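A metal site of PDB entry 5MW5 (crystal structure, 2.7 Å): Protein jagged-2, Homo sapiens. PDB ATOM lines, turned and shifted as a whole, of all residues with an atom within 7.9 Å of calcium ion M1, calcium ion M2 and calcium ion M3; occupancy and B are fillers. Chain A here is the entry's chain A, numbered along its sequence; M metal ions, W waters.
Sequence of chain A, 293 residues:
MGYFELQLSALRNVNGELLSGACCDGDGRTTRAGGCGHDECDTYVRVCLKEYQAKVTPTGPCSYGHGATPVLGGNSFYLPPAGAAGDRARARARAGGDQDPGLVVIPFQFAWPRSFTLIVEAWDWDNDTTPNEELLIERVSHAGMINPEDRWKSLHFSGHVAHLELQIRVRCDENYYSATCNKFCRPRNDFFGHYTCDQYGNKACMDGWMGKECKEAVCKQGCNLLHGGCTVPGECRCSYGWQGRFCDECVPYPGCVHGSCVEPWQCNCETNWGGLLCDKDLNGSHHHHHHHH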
ATOM      1  N   LEU A  18     -20.939  27.424   8.618  1.00  0.00           N
ATOM      2  CA  LEU A  18     -19.840  28.137   7.996  1.00  0.00           C
ATOM      3  C   LEU A  18     -19.072  28.918   9.068  1.00  0.00           C
ATOM      4  O   LEU A  18     -19.482  28.991  10.226  1.00  0.00           O
ATOM      5  CB  LEU A  18     -20.336  29.084   6.895  1.00  0.00           C
ATOM      6  CG  LEU A  18     -21.320  28.527   5.859  1.00  0.00           C
ATOM      7  CD1 LEU A  18     -22.626  29.286   5.934  1.00  0.00           C
ATOM      8  CD2 LEU A  18     -20.746  28.581   4.453  1.00  0.00           C
ATOM      9  N   CYS A  23     -25.914  28.968   8.798  1.00  0.00           N
ATOM     10  CA  CYS A  23     -26.070  27.680   8.160  1.00  0.00           C
ATOM     11  C   CYS A  23     -25.743  27.795   6.677  1.00  0.00           C
ATOM     12  O   CYS A  23     -25.960  28.843   6.051  1.00  0.00           O
ATOM     13  CB  CYS A  23     -27.493  27.145   8.351  1.00  0.00           C
ATOM     14  SG  CYS A  23     -27.970  26.840  10.073  1.00  0.00           S
ATOM     15  N   CYS A  24     -25.223  26.703   6.110  1.00  0.00           N
ATOM     16  CA  CYS A  24     -24.794  26.719   4.715  1.00  0.00           C
ATOM     17  C   CYS A  24     -25.958  27.027   3.781  1.00  0.00           C
ATOM     18  O   CYS A  24     -25.929  28.016   3.026  1.00  0.00           O
ATOM     19  CB  CYS A  24     -24.158  25.382   4.356  1.00  0.00           C
ATOM     20  SG  CYS A  24     -22.477  25.155   4.960  1.00  0.00           S
ATOM     21  N   ASP A  25     -26.992  26.207   3.815  1.00  0.00           N
ATOM     22  CA  ASP A  25     -28.147  26.390   2.949  1.00  0.00           C
ATOM     23  C   ASP A  25     -29.446  26.391   3.747  1.00  0.00           C
ATOM     24  O   ASP A  25     -30.008  27.443   4.026  1.00  0.00           O
ATOM     25  CB  ASP A  25     -28.173  25.305   1.873  1.00  0.00           C
ATOM     26  CG  ASP A  25     -26.903  25.265   1.051  1.00  0.00           C
ATOM     27  OD1 ASP A  25     -26.228  26.311   0.951  1.00  0.00           O
ATOM     28  OD2 ASP A  25     -26.574  24.193   0.501  1.00  0.00           O
ATOM     29  N   HIS A  38     -31.525  20.296   6.828  1.00  0.00           N
ATOM     30  CA  HIS A  38     -31.175  19.128   6.023  1.00  0.00           C
ATOM     31  C   HIS A  38     -30.523  19.449   4.689  1.00  0.00           C
ATOM     32  O   HIS A  38     -29.831  18.584   4.148  1.00  0.00           O
ATOM     33  CB  HIS A  38     -32.420  18.268   5.757  1.00  0.00           C
ATOM     34  CG  HIS A  38     -32.684  17.238   6.821  1.00  0.00           C
ATOM     35  ND1 HIS A  38     -31.763  16.265   7.146  1.00  0.00           N
ATOM     36  CD2 HIS A  38     -33.753  17.046   7.622  1.00  0.00           C
ATOM     37  CE1 HIS A  38     -32.263  15.511   8.112  1.00  0.00           C
ATOM     38  NE2 HIS A  38     -33.462  15.960   8.412  1.00  0.00           N
ATOM     39  N   ASP A  39     -30.713  20.652   4.140  1.00  0.00           N
ATOM     40  CA  ASP A  39     -29.978  21.072   2.947  1.00  0.00           C
ATOM     41  C   ASP A  39     -28.523  21.305   3.342  1.00  0.00           C
ATOM     42  O   ASP A  39     -28.181  22.350   3.896  1.00  0.00           O
ATOM     43  CB  ASP A  39     -30.611  22.314   2.343  1.00  0.00           C
ATOM     44  CG  ASP A  39     -30.041  22.668   0.978  1.00  0.00           C
ATOM     45  OD1 ASP A  39     -29.168  21.933   0.483  1.00  0.00           O
ATOM     46  OD2 ASP A  39     -30.489  23.675   0.391  1.00  0.00           O
ATOM     47  N   GLU A  40     -27.668  20.317   3.073  1.00  0.00           N
ATOM     48  CA  GLU A  40     -26.330  20.298   3.643  1.00  0.00           C
ATOM     49  C   GLU A  40     -25.408  21.280   2.929  1.00  0.00           C
ATOM     50  O   GLU A  40     -25.745  21.869   1.904  1.00  0.00           O
ATOM     51  CB  GLU A  40     -25.739  18.892   3.570  1.00  0.00           C
ATOM     52  CG  GLU A  40     -26.635  17.810   4.142  1.00  0.00           C
ATOM     53  CD  GLU A  40     -25.861  16.848   5.019  1.00  0.00           C
ATOM     54  OE1 GLU A  40     -26.511  16.070   5.757  1.00  0.00           O
ATOM     55  OE2 GLU A  40     -24.608  16.875   4.991  1.00  0.00           O
ATOM     56  N   CYS A  41     -24.217  21.428   3.502  1.00  0.00           N
ATOM     57  CA  CYS A  41     -23.152  22.165   2.831  1.00  0.00           C
ATOM     58  C   CYS A  41     -22.679  21.378   1.616  1.00  0.00           C
ATOM     59  O   CYS A  41     -22.481  20.157   1.693  1.00  0.00           O
ATOM     60  CB  CYS A  41     -21.981  22.406   3.790  1.00  0.00           C
ATOM     61  SG  CYS A  41     -22.418  23.163   5.361  1.00  0.00           S
ATOM     62  N   ASP A  42     -22.523  22.059   0.492  1.00  0.00           N
ATOM     63  CA  ASP A  42     -22.006  21.442  -0.731  1.00  0.00           C
ATOM     64  C   ASP A  42     -20.521  21.773  -0.779  1.00  0.00           C
ATOM     65  O   ASP A  42     -20.100  22.778  -1.354  1.00  0.00           O
ATOM     66  CB  ASP A  42     -22.775  21.939  -1.945  1.00  0.00           C
ATOM     67  CG  ASP A  42     -24.277  22.060  -1.670  1.00  0.00           C
ATOM     68  OD1 ASP A  42     -24.945  21.024  -1.474  1.00  0.00           O
ATOM     69  OD2 ASP A  42     -24.783  23.204  -1.644  1.00  0.00           O
ATOM     70  N   THR A  43     -19.720  20.901  -0.174  1.00  0.00           N
ATOM     71  CA  THR A  43     -18.366  21.236   0.240  1.00  0.00           C
ATOM     72  C   THR A  43     -17.346  20.966  -0.867  1.00  0.00           C
ATOM     73  O   THR A  43     -17.324  19.878  -1.448  1.00  0.00           O
ATOM     74  CB  THR A  43     -17.988  20.436   1.487  1.00  0.00           C
ATOM     75  OG1 THR A  43     -18.959  20.675   2.522  1.00  0.00           O
ATOM     76  CG2 THR A  43     -16.612  20.833   1.994  1.00  0.00           C
ATOM     77  N   GLY A  73     -18.814  16.243  -1.019  1.00  0.00           N
ATOM     78  CA  GLY A  73     -19.816  15.654  -0.162  1.00  0.00           C
ATOM     79  C   GLY A  73     -20.595  16.713   0.584  1.00  0.00           C
ATOM     80  O   GLY A  73     -20.557  17.899   0.256  1.00  0.00           O
ATOM     81  N   GLY A  74     -21.324  16.254   1.601  1.00  0.00           N
ATOM     82  CA  GLY A  74     -22.192  17.117   2.369  1.00  0.00           C
ATOM     83  C   GLY A  74     -21.518  17.776   3.551  1.00  0.00           C
ATOM     84  O   GLY A  74     -20.781  18.757   3.399  1.00  0.00           O
ATOM     85  N   TRP A 123     -15.375  25.289   1.410  1.00  0.00           N
ATOM     86  CA  TRP A 123     -16.382  26.203   0.896  1.00  0.00           C
ATOM     87  C   TRP A 123     -17.679  25.472   0.618  1.00  0.00           C
ATOM     88  O   TRP A 123     -17.672  24.316   0.187  1.00  0.00           O
ATOM     89  CB  TRP A 123     -15.913  26.889  -0.390  1.00  0.00           C
ATOM     90  CG  TRP A 123     -14.783  27.854  -0.214  1.00  0.00           C
ATOM     91  CD1 TRP A 123     -13.463  27.544  -0.068  1.00  0.00           C
ATOM     92  CD2 TRP A 123     -14.868  29.283  -0.178  1.00  0.00           C
ATOM     93  NE1 TRP A 123     -12.724  28.689   0.059  1.00  0.00           N
ATOM     94  CE2 TRP A 123     -13.566  29.777   0.000  1.00  0.00           C
ATOM     95  CE3 TRP A 123     -15.923  30.189  -0.272  1.00  0.00           C
ATOM     96  CZ2 TRP A 123     -13.284  31.130   0.080  1.00  0.00           C
ATOM     97  CZ3 TRP A 123     -15.642  31.542  -0.192  1.00  0.00           C
ATOM     98  CH2 TRP A 123     -14.339  32.000  -0.020  1.00  0.00           C
ATOM     99  N   ASP A 124     -18.791  26.158   0.848  1.00  0.00           N
ATOM    100  CA  ASP A 124     -20.098  25.713   0.362  1.00  0.00           C
ATOM    101  C   ASP A 124     -20.354  26.339  -1.000  1.00  0.00           C
ATOM    102  O   ASP A 124     -20.249  27.566  -1.159  1.00  0.00           O
ATOM    103  CB  ASP A 124     -21.218  26.089   1.341  1.00  0.00           C
ATOM    104  CG  ASP A 124     -22.604  25.860   0.748  1.00  0.00           C
ATOM    105  OD1 ASP A 124     -23.047  24.695   0.698  1.00  0.00           O
ATOM    106  OD2 ASP A 124     -23.261  26.848   0.358  1.00  0.00           O
ATOM    107  N   TRP A 125     -20.672  25.500  -1.980  1.00  0.00           N
ATOM    108  CA  TRP A 125     -21.076  25.953  -3.297  1.00  0.00           C
ATOM    109  C   TRP A 125     -22.588  26.144  -3.307  1.00  0.00           C
ATOM    110  O   TRP A 125     -23.333  25.409  -2.655  1.00  0.00           O
ATOM    111  CB  TRP A 125     -20.623  24.948  -4.357  1.00  0.00           C
ATOM    112  CG  TRP A 125     -21.257  25.116  -5.695  1.00  0.00           C
ATOM    113  CD1 TRP A 125     -20.757  25.804  -6.755  1.00  0.00           C
ATOM    114  CD2 TRP A 125     -22.505  24.566  -6.121  1.00  0.00           C
ATOM    115  NE1 TRP A 125     -21.621  25.724  -7.824  1.00  0.00           N
ATOM    116  CE2 TRP A 125     -22.702  24.964  -7.452  1.00  0.00           C
ATOM    117  CE3 TRP A 125     -23.478  23.782  -5.501  1.00  0.00           C
ATOM    118  CZ2 TRP A 125     -23.834  24.605  -8.172  1.00  0.00           C
ATOM    119  CZ3 TRP A 125     -24.596  23.425  -6.212  1.00  0.00           C
ATOM    120  CH2 TRP A 125     -24.770  23.841  -7.538  1.00  0.00           C
ATOM    121  N   ASP A 126     -23.053  27.152  -4.064  1.00  0.00           N
ATOM    122  CA  ASP A 126     -24.413  27.629  -3.906  1.00  0.00           C
ATOM    123  C   ASP A 126     -25.213  27.843  -5.186  1.00  0.00           C
ATOM    124  O   ASP A 126     -26.332  28.361  -5.116  1.00  0.00           O
ATOM    125  CB  ASP A 126     -24.417  28.952  -3.120  1.00  0.00           C
ATOM    126  CG  ASP A 126     -24.831  28.775  -1.680  1.00  0.00           C
ATOM    127  OD1 ASP A 126     -24.886  27.612  -1.232  1.00  0.00           O
ATOM    128  OD2 ASP A 126     -25.108  29.778  -1.001  1.00  0.00           O
ATOM    129  N   ASN A 127     -24.674  27.451  -6.350  1.00  0.00           N
ATOM    130  CA  ASN A 127     -25.346  27.666  -7.638  1.00  0.00           C
ATOM    131  C   ASN A 127     -25.650  29.156  -7.845  1.00  0.00           C
ATOM    132  O   ASN A 127     -26.801  29.604  -7.842  1.00  0.00           O
ATOM    133  CB  ASN A 127     -26.613  26.815  -7.749  1.00  0.00           C
ATOM    134  CG  ASN A 127     -27.349  27.015  -9.062  1.00  0.00           C
ATOM    135  OD1 ASN A 127     -26.761  27.408 -10.068  1.00  0.00           O
ATOM    136  ND2 ASN A 127     -28.654  26.746  -9.063  1.00  0.00           N
ATOM    137  N   ASN A 132     -19.391  35.027  -3.916  1.00  0.00           N
ATOM    138  CA  ASN A 132     -19.813  35.339  -2.548  1.00  0.00           C
ATOM    139  C   ASN A 132     -18.781  34.760  -1.584  1.00  0.00           C
ATOM    140  O   ASN A 132     -18.717  33.547  -1.382  1.00  0.00           O
ATOM    141  CB  ASN A 132     -21.204  34.768  -2.291  1.00  0.00           C
ATOM    142  CG  ASN A 132     -21.724  35.083  -0.897  1.00  0.00           C
ATOM    143  OD1 ASN A 132     -21.108  35.831  -0.136  1.00  0.00           O
ATOM    144  ND2 ASN A 132     -22.871  34.499  -0.557  1.00  0.00           N
ATOM    145  N   GLU A 134     -18.644  35.114   1.637  1.00  0.00           N
ATOM    146  CA  GLU A 134     -19.234  34.770   2.932  1.00  0.00           C
ATOM    147  C   GLU A 134     -19.490  33.268   3.052  1.00  0.00           C
ATOM    148  O   GLU A 134     -19.789  32.769   4.145  1.00  0.00           O
ATOM    149  CB  GLU A 134     -20.531  35.561   3.140  1.00  0.00           C
ATOM    150  CG  GLU A 134     -21.096  35.480   4.559  1.00  0.00           C
ATOM    151  CD  GLU A 134     -21.927  36.688   4.940  1.00  0.00           C
ATOM    152  OE1 GLU A 134     -21.695  37.241   6.031  1.00  0.00           O
ATOM    153  OE2 GLU A 134     -22.826  37.067   4.159  1.00  0.00           O
ATOM    154  N   LEU A 135     -19.372  32.535   1.943  1.00  0.00           N
ATOM    155  CA  LEU A 135     -19.625  31.108   1.911  1.00  0.00           C
ATOM    156  C   LEU A 135     -18.418  30.279   2.327  1.00  0.00           C
ATOM    157  O   LEU A 135     -18.283  29.122   1.889  1.00  0.00           O
ATOM    158  CB  LEU A 135     -20.081  30.698   0.511  1.00  0.00           C
ATOM    159  CG  LEU A 135     -21.439  31.252   0.055  1.00  0.00           C
ATOM    160  CD1 LEU A 135     -21.695  30.892  -1.402  1.00  0.00           C
ATOM    161  CD2 LEU A 135     -22.543  30.716   0.942  1.00  0.00           C
HETATM  162 CA    CA M   1     -25.078  28.370   0.913  1.00  0.00          CA
HETATM  163 CA    CA M   2     -26.849  21.933  -0.228  1.00  0.00          CA
HETATM  164 CA    CA M   3     -24.831  25.346  -0.678  1.00  0.00          CA
HETATM  165  O   HOH W   1     -27.295  19.539  -0.162  1.00  0.00           O
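Calcium ion M1 is bound by the side-chain carboxylate (OD1) of Asp 126, the backbone carbonyl oxygen (O) of Cys 24, the side-chain carboxylate (OD1) of Asp 25, the side-chain carboxylate (OD2) of Asp 126 and the side-chain carboxylate (OD2) of Asp 124. Calcium ion M1 has five donor atoms within binding distance.
Five residues have an atom within 4 Å of calcium ion M3: Asp 25, Asp 42, Asp 124, Trp 125 and Asp 126.
Calcium ion M3 is bound by OD1 of Asp 126. The side-chain carboxylate (OD1) of Asp 124 binds calcium ion M3. OD2 of Asp 42 binds calcium ion M3, 2.4 Å away. OD1 of Asp 25 is bound to calcium ion M3, at 2.4 Å. OD2 of Asp 25 binds calcium ion M3, 2.4 Å away. Calcium ion M3 is bound by the side-chain carboxylate (OD2) of Asp 124 (2.4 Å). The backbone carbonyl oxygen (O) of Trp 125 is bound to calcium ion M3 (2.5 Å).
SG of Cys 41 is disulfide-bonded to SG of Cys 24 (2.0 Å). O of Leu 135 is in hydrogen-bond range of N of Asp 124 (3.2 Å).
Calcium ion M2 is bound by the side-chain carboxylate (OD2) of Asp 25 (2.4 Å), the backbone carbonyl oxygen (O) of Glu 40 (2.4 Å), the side-chain carboxylate (OD1) of Asp 39 (2.4 Å), water W1 (2.4 Å), the side-chain carboxylate (OD1) of Asp 42 (2.5 Å) and the side-chain carboxylate (OD2) of Asp 42 (2.8 Å). Calcium ion M2 has six donor atoms within binding distance.
Leu 135 touches calcium ion M1. Of the 20 residues printed, 5 come within 4 Å of calcium ion M1. Along chain A the residues within 4 Å of calcium ion M1 span positions 24 to 135.
Of the 20 residues printed, 4 come within 4 Å of calcium ion M2. The nearest printed residue that does not touch calcium ion M2 is Cys 41 (4.6 Å).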
